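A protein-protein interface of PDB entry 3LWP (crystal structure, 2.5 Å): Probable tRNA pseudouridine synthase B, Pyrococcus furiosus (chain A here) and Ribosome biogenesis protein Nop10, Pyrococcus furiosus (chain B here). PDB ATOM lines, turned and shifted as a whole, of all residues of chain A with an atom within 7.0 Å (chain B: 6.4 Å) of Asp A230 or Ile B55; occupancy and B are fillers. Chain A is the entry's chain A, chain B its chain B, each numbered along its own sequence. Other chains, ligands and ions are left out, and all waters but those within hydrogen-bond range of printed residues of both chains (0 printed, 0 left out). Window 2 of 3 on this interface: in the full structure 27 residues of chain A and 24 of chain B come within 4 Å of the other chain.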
ATOM      1  N   ASP A 222      11.651 -16.881  13.341  1.00  0.00           N
ATOM      2  CA  ASP A 222      10.677 -17.663  14.083  1.00  0.00           C
ATOM      3  C   ASP A 222      10.692 -17.378  15.608  1.00  0.00           C
ATOM      4  O   ASP A 222       9.644 -17.209  16.218  1.00  0.00           O
ATOM      5  CB  ASP A 222      10.841 -19.149  13.790  1.00  0.00           C
ATOM      6  CG  ASP A 222      10.495 -19.495  12.321  1.00  0.00           C
ATOM      7  OD1 ASP A 222      10.079 -18.590  11.604  1.00  0.00           O
ATOM      8  OD2 ASP A 222      10.649 -20.657  11.882  1.00  0.00           O
ATOM      9  N   TYR A 224      11.656 -14.750  17.011  1.00  0.00           N
ATOM     10  CA  TYR A 224      11.093 -13.424  17.109  1.00  0.00           C
ATOM     11  C   TYR A 224       9.574 -13.493  17.206  1.00  0.00           C
ATOM     12  O   TYR A 224       8.996 -12.960  18.147  1.00  0.00           O
ATOM     13  CB  TYR A 224      11.526 -12.555  15.937  1.00  0.00           C
ATOM     14  CG  TYR A 224      10.879 -11.193  15.923  1.00  0.00           C
ATOM     15  CD1 TYR A 224      11.287 -10.183  16.810  1.00  0.00           C
ATOM     16  CD2 TYR A 224       9.872 -10.893  14.994  1.00  0.00           C
ATOM     17  CE1 TYR A 224      10.697  -8.894  16.767  1.00  0.00           C
ATOM     18  CE2 TYR A 224       9.280  -9.650  14.952  1.00  0.00           C
ATOM     19  CZ  TYR A 224       9.685  -8.646  15.834  1.00  0.00           C
ATOM     20  OH  TYR A 224       9.056  -7.410  15.762  1.00  0.00           O
ATOM     21  N   TYR A 225       8.938 -14.179  16.259  1.00  0.00           N
ATOM     22  CA  TYR A 225       7.482 -14.324  16.275  1.00  0.00           C
ATOM     23  C   TYR A 225       6.960 -15.063  17.500  1.00  0.00           C
ATOM     24  O   TYR A 225       5.940 -14.670  18.069  1.00  0.00           O
ATOM     25  CB  TYR A 225       6.977 -14.992  15.000  1.00  0.00           C
ATOM     26  CG  TYR A 225       7.004 -14.046  13.836  1.00  0.00           C
ATOM     27  CD1 TYR A 225       7.739 -14.344  12.698  1.00  0.00           C
ATOM     28  CD2 TYR A 225       6.315 -12.832  13.885  1.00  0.00           C
ATOM     29  CE1 TYR A 225       7.778 -13.477  11.629  1.00  0.00           C
ATOM     30  CE2 TYR A 225       6.352 -11.945  12.823  1.00  0.00           C
ATOM     31  CZ  TYR A 225       7.090 -12.279  11.691  1.00  0.00           C
ATOM     32  OH  TYR A 225       7.144 -11.426  10.613  1.00  0.00           O
ATOM     33  N   PHE A 226       7.654 -16.127  17.900  1.00  0.00           N
ATOM     34  CA  PHE A 226       7.338 -16.816  19.149  1.00  0.00           C
ATOM     35  C   PHE A 226       7.306 -15.866  20.323  1.00  0.00           C
ATOM     36  O   PHE A 226       6.571 -16.080  21.278  1.00  0.00           O
ATOM     37  CB  PHE A 226       8.345 -17.912  19.461  1.00  0.00           C
ATOM     38  CG  PHE A 226       8.314 -19.029  18.492  1.00  0.00           C
ATOM     39  CD1 PHE A 226       9.326 -19.958  18.467  1.00  0.00           C
ATOM     40  CD2 PHE A 226       7.291 -19.107  17.554  1.00  0.00           C
ATOM     41  CE1 PHE A 226       9.304 -21.001  17.544  1.00  0.00           C
ATOM     42  CE2 PHE A 226       7.261 -20.131  16.629  1.00  0.00           C
ATOM     43  CZ  PHE A 226       8.271 -21.086  16.625  1.00  0.00           C
ATOM     44  N   TRP A 227       8.123 -14.826  20.254  1.00  0.00           N
ATOM     45  CA  TRP A 227       8.132 -13.833  21.295  1.00  0.00           C
ATOM     46  C   TRP A 227       7.017 -12.810  21.088  1.00  0.00           C
ATOM     47  O   TRP A 227       6.244 -12.543  22.000  1.00  0.00           O
ATOM     48  CB  TRP A 227       9.500 -13.177  21.419  1.00  0.00           C
ATOM     49  CG  TRP A 227       9.504 -11.968  22.222  1.00  0.00           C
ATOM     50  CD1 TRP A 227       9.022 -11.823  23.500  1.00  0.00           C
ATOM     51  CD2 TRP A 227      10.018 -10.691  21.834  1.00  0.00           C
ATOM     52  NE1 TRP A 227       9.201 -10.516  23.924  1.00  0.00           N
ATOM     53  CE2 TRP A 227       9.786  -9.796  22.917  1.00  0.00           C
ATOM     54  CE3 TRP A 227      10.631 -10.205  20.674  1.00  0.00           C
ATOM     55  CZ2 TRP A 227      10.163  -8.453  22.875  1.00  0.00           C
ATOM     56  CZ3 TRP A 227      11.008  -8.845  20.628  1.00  0.00           C
ATOM     57  CH2 TRP A 227      10.768  -7.992  21.722  1.00  0.00           C
ATOM     58  N   LYS A 228       6.911 -12.272  19.884  1.00  0.00           N
ATOM     59  CA  LYS A 228       6.001 -11.148  19.633  1.00  0.00           C
ATOM     60  C   LYS A 228       4.518 -11.558  19.660  1.00  0.00           C
ATOM     61  O   LYS A 228       3.666 -10.819  20.170  1.00  0.00           O
ATOM     62  CB  LYS A 228       6.331 -10.479  18.298  1.00  0.00           C
ATOM     63  CG  LYS A 228       6.599  -8.990  18.403  1.00  0.00           C
ATOM     64  CD  LYS A 228       7.785  -8.699  19.289  1.00  0.00           C
ATOM     65  CE  LYS A 228       7.962  -7.174  19.526  1.00  0.00           C
ATOM     66  NZ  LYS A 228       6.708  -6.305  19.465  1.00  0.00           N
ATOM     67  N   GLU A 229       4.239 -12.751  19.146  1.00  0.00           N
ATOM     68  CA  GLU A 229       2.888 -13.208  18.841  1.00  0.00           C
ATOM     69  C   GLU A 229       2.385 -14.311  19.757  1.00  0.00           C
ATOM     70  O   GLU A 229       1.164 -14.494  19.889  1.00  0.00           O
ATOM     71  CB  GLU A 229       2.824 -13.700  17.393  1.00  0.00           C
ATOM     72  CG  GLU A 229       2.911 -12.574  16.378  1.00  0.00           C
ATOM     73  CD  GLU A 229       2.768 -13.079  14.950  1.00  0.00           C
ATOM     74  OE1 GLU A 229       2.646 -12.229  14.027  1.00  0.00           O
ATOM     75  OE2 GLU A 229       2.773 -14.325  14.766  1.00  0.00           O
ATOM     76  N   ASP A 230       3.320 -15.026  20.380  1.00  0.00           N
ATOM     77  CA  ASP A 230       3.015 -16.147  21.252  1.00  0.00           C
ATOM     78  C   ASP A 230       3.402 -15.884  22.700  1.00  0.00           C
ATOM     79  O   ASP A 230       3.088 -16.683  23.578  1.00  0.00           O
ATOM     80  CB  ASP A 230       3.761 -17.398  20.786  1.00  0.00           C
ATOM     81  CG  ASP A 230       3.248 -17.928  19.468  1.00  0.00           C
ATOM     82  OD1 ASP A 230       2.072 -18.342  19.432  1.00  0.00           O
ATOM     83  OD2 ASP A 230       4.020 -17.955  18.482  1.00  0.00           O
ATOM     84  N   GLY A 231       4.114 -14.794  22.955  1.00  0.00           N
ATOM     85  CA  GLY A 231       4.490 -14.436  24.315  1.00  0.00           C
ATOM     86  C   GLY A 231       5.645 -15.226  24.935  1.00  0.00           C
ATOM     87  O   GLY A 231       5.907 -15.093  26.137  1.00  0.00           O
ATOM     88  N   ILE A 232       6.328 -16.048  24.140  1.00  0.00           N
ATOM     89  CA  ILE A 232       7.494 -16.787  24.630  1.00  0.00           C
ATOM     90  C   ILE A 232       8.764 -16.024  24.313  1.00  0.00           C
ATOM     91  O   ILE A 232       9.070 -15.732  23.150  1.00  0.00           O
ATOM     92  CB  ILE A 232       7.612 -18.192  24.042  1.00  0.00           C
ATOM     93  CG1 ILE A 232       6.251 -18.879  24.026  1.00  0.00           C
ATOM     94  CG2 ILE A 232       8.618 -19.000  24.848  1.00  0.00           C
ATOM     95  CD1 ILE A 232       5.425 -18.586  25.265  1.00  0.00           C
ATOM     96  N   GLU A 233       9.500 -15.707  25.366  1.00  0.00           N
ATOM     97  CA  GLU A 233      10.625 -14.785  25.281  1.00  0.00           C
ATOM     98  C   GLU A 233      11.942 -15.567  25.210  1.00  0.00           C
ATOM     99  O   GLU A 233      12.958 -15.067  24.714  1.00  0.00           O
ATOM    100  CB  GLU A 233      10.591 -13.848  26.498  1.00  0.00           C
ATOM    101  CG  GLU A 233      11.803 -12.932  26.674  1.00  0.00           C
ATOM    102  CD  GLU A 233      11.869 -12.258  28.070  1.00  0.00           C
ATOM    103  OE1 GLU A 233      10.953 -11.459  28.396  1.00  0.00           O
ATOM    104  OE2 GLU A 233      12.854 -12.515  28.825  1.00  0.00           O
ATOM    105  N   TYR A 235      13.343 -18.137  23.516  1.00  0.00           N
ATOM    106  CA  TYR A 235      14.133 -18.430  22.324  1.00  0.00           C
ATOM    107  C   TYR A 235      14.714 -17.158  21.717  1.00  0.00           C
ATOM    108  O   TYR A 235      15.887 -17.102  21.368  1.00  0.00           O
ATOM    109  CB  TYR A 235      13.327 -19.240  21.309  1.00  0.00           C
ATOM    110  CG  TYR A 235      12.732 -20.468  21.934  1.00  0.00           C
ATOM    111  CD1 TYR A 235      11.391 -20.497  22.312  1.00  0.00           C
ATOM    112  CD2 TYR A 235      13.514 -21.585  22.197  1.00  0.00           C
ATOM    113  CE1 TYR A 235      10.843 -21.620  22.916  1.00  0.00           C
ATOM    114  CE2 TYR A 235      12.972 -22.713  22.809  1.00  0.00           C
ATOM    115  CZ  TYR A 235      11.635 -22.724  23.165  1.00  0.00           C
ATOM    116  OH  TYR A 235      11.083 -23.843  23.761  1.00  0.00           O
ATOM    117  N   LYS B  49       7.542 -26.128  13.803  1.00  0.00           N
ATOM    118  CA  LYS B  49       8.662 -25.891  14.687  1.00  0.00           C
ATOM    119  C   LYS B  49       8.210 -25.818  16.154  1.00  0.00           C
ATOM    120  O   LYS B  49       8.921 -26.262  17.047  1.00  0.00           O
ATOM    121  CB  LYS B  49       9.344 -24.610  14.258  1.00  0.00           C
ATOM    122  CG  LYS B  49      10.644 -24.341  14.921  1.00  0.00           C
ATOM    123  CD  LYS B  49      11.323 -23.124  14.292  1.00  0.00           C
ATOM    124  CE  LYS B  49      12.125 -23.499  13.015  1.00  0.00           C
ATOM    125  NZ  LYS B  49      12.938 -22.339  12.496  1.00  0.00           N
ATOM    126  N   ARG B  50       7.029 -25.253  16.394  1.00  0.00           N
ATOM    127  CA  ARG B  50       6.427 -25.265  17.727  1.00  0.00           C
ATOM    128  C   ARG B  50       6.273 -26.692  18.216  1.00  0.00           C
ATOM    129  O   ARG B  50       6.663 -27.016  19.336  1.00  0.00           O
ATOM    130  CB  ARG B  50       5.057 -24.583  17.720  1.00  0.00           C
ATOM    131  CG  ARG B  50       5.143 -23.096  17.485  1.00  0.00           C
ATOM    132  CD  ARG B  50       3.799 -22.432  17.704  1.00  0.00           C
ATOM    133  NE  ARG B  50       3.855 -21.019  17.352  1.00  0.00           N
ATOM    134  CZ  ARG B  50       3.372 -20.536  16.217  1.00  0.00           C
ATOM    135  NH1 ARG B  50       2.779 -21.372  15.377  1.00  0.00           N
ATOM    136  NH2 ARG B  50       3.465 -19.232  15.936  1.00  0.00           N
ATOM    137  N   GLU B  51       5.713 -27.546  17.367  1.00  0.00           N
ATOM    138  CA  GLU B  51       5.495 -28.927  17.731  1.00  0.00           C
ATOM    139  C   GLU B  51       6.824 -29.558  18.150  1.00  0.00           C
ATOM    140  O   GLU B  51       6.913 -30.208  19.200  1.00  0.00           O
ATOM    141  CB  GLU B  51       4.835 -29.686  16.580  1.00  0.00           C
ATOM    142  CG  GLU B  51       4.197 -31.013  16.998  1.00  0.00           C
ATOM    143  CD  GLU B  51       2.932 -31.353  16.192  1.00  0.00           C
ATOM    144  OE1 GLU B  51       2.356 -30.436  15.553  1.00  0.00           O
ATOM    145  OE2 GLU B  51       2.509 -32.534  16.206  1.00  0.00           O
ATOM    146  N   VAL B  52       7.859 -29.336  17.339  1.00  0.00           N
ATOM    147  CA  VAL B  52       9.206 -29.842  17.627  1.00  0.00           C
ATOM    148  C   VAL B  52       9.689 -29.307  18.973  1.00  0.00           C
ATOM    149  O   VAL B  52      10.064 -30.080  19.846  1.00  0.00           O
ATOM    150  CB  VAL B  52      10.225 -29.467  16.481  1.00  0.00           C
ATOM    151  CG1 VAL B  52      11.647 -29.553  16.954  1.00  0.00           C
ATOM    152  CG2 VAL B  52      10.014 -30.331  15.215  1.00  0.00           C
ATOM    153  N   LEU B  53       9.668 -27.988  19.138  1.00  0.00           N
ATOM    154  CA  LEU B  53      10.109 -27.349  20.382  1.00  0.00           C
ATOM    155  C   LEU B  53       9.235 -27.643  21.613  1.00  0.00           C
ATOM    156  O   LEU B  53       9.755 -27.882  22.703  1.00  0.00           O
ATOM    157  CB  LEU B  53      10.229 -25.834  20.203  1.00  0.00           C
ATOM    158  CG  LEU B  53      11.271 -25.362  19.199  1.00  0.00           C
ATOM    159  CD1 LEU B  53      11.287 -23.842  19.128  1.00  0.00           C
ATOM    160  CD2 LEU B  53      12.637 -25.906  19.587  1.00  0.00           C
ATOM    161  N   GLY B  54       7.917 -27.599  21.445  1.00  0.00           N
ATOM    162  CA  GLY B  54       6.995 -27.868  22.537  1.00  0.00           C
ATOM    163  C   GLY B  54       6.326 -26.635  23.115  1.00  0.00           C
ATOM    164  O   GLY B  54       5.960 -26.618  24.287  1.00  0.00           O
ATOM    165  N   ILE B  55       6.160 -25.594  22.306  1.00  0.00           N
ATOM    166  CA  ILE B  55       5.492 -24.385  22.786  1.00  0.00           C
ATOM    167  C   ILE B  55       3.979 -24.492  22.607  1.00  0.00           C
ATOM    168  O   ILE B  55       3.505 -25.339  21.847  1.00  0.00           O
ATOM    169  CB  ILE B  55       5.990 -23.100  22.081  1.00  0.00           C
ATOM    170  CG1 ILE B  55       4.971 -22.636  21.040  1.00  0.00           C
ATOM    171  CG2 ILE B  55       7.410 -23.277  21.501  1.00  0.00           C
ATOM    172  CD1 ILE B  55       4.928 -21.117  20.858  1.00  0.00           C
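Of chain B, only Arg B50 (2.9 Å) and Ile B55 (3.9 Å) come within 4 Å of Asp A230.
Ile B55 touches one residue of chain A.
Of the printed residues of chain A, Lys B49 touches Asp A222 (2.9 Å).
Of the printed residues of chain A, Arg B50 touches Phe A226 (3.6 Å) and Asp A230 (2.9 Å).
Glu A233 touches none of the printed residues of chain B.
The nearest residue of chain A that does not touch Ile B55 is Tyr A235 (4.1 Å).
Hydrophobic or aromatic side chains of chain A that line the printed part of chain B: Phe A226.
Among the printed residues, Asp or Glu carboxylates within 4 Å of a Lys or Arg side-chain nitrogen of the other chain: Asp A222 with Lys B49 (2.9 Å) and Asp A230 with Arg B50 (2.9 Å).
OD2 of Asp A222 lies within salt-bridge range of NZ of Lys B49, at 2.9 Å.
The side-chain carboxylate (OD2) of Asp A230 lies within salt-bridge range of the guanidinium group (NH2) of Arg B50.
Phe A226 touches Arg B50.
Phe A226 touches Leu B53.
Asp A230 touches Ile B55.
O of Phe A226 lies within hydrogen-bond range of N of Gly A231, at 3.2 Å.
The backbone carbonyl oxygen of Phe A226 lies within hydrogen-bond range of the backbone NH of Ile A232 (2.9 Å).
The backbone carbonyl oxygen of Arg B50 sits at hydrogen-bond distance from the backbone NH of Ile B55 (3.3 Å).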
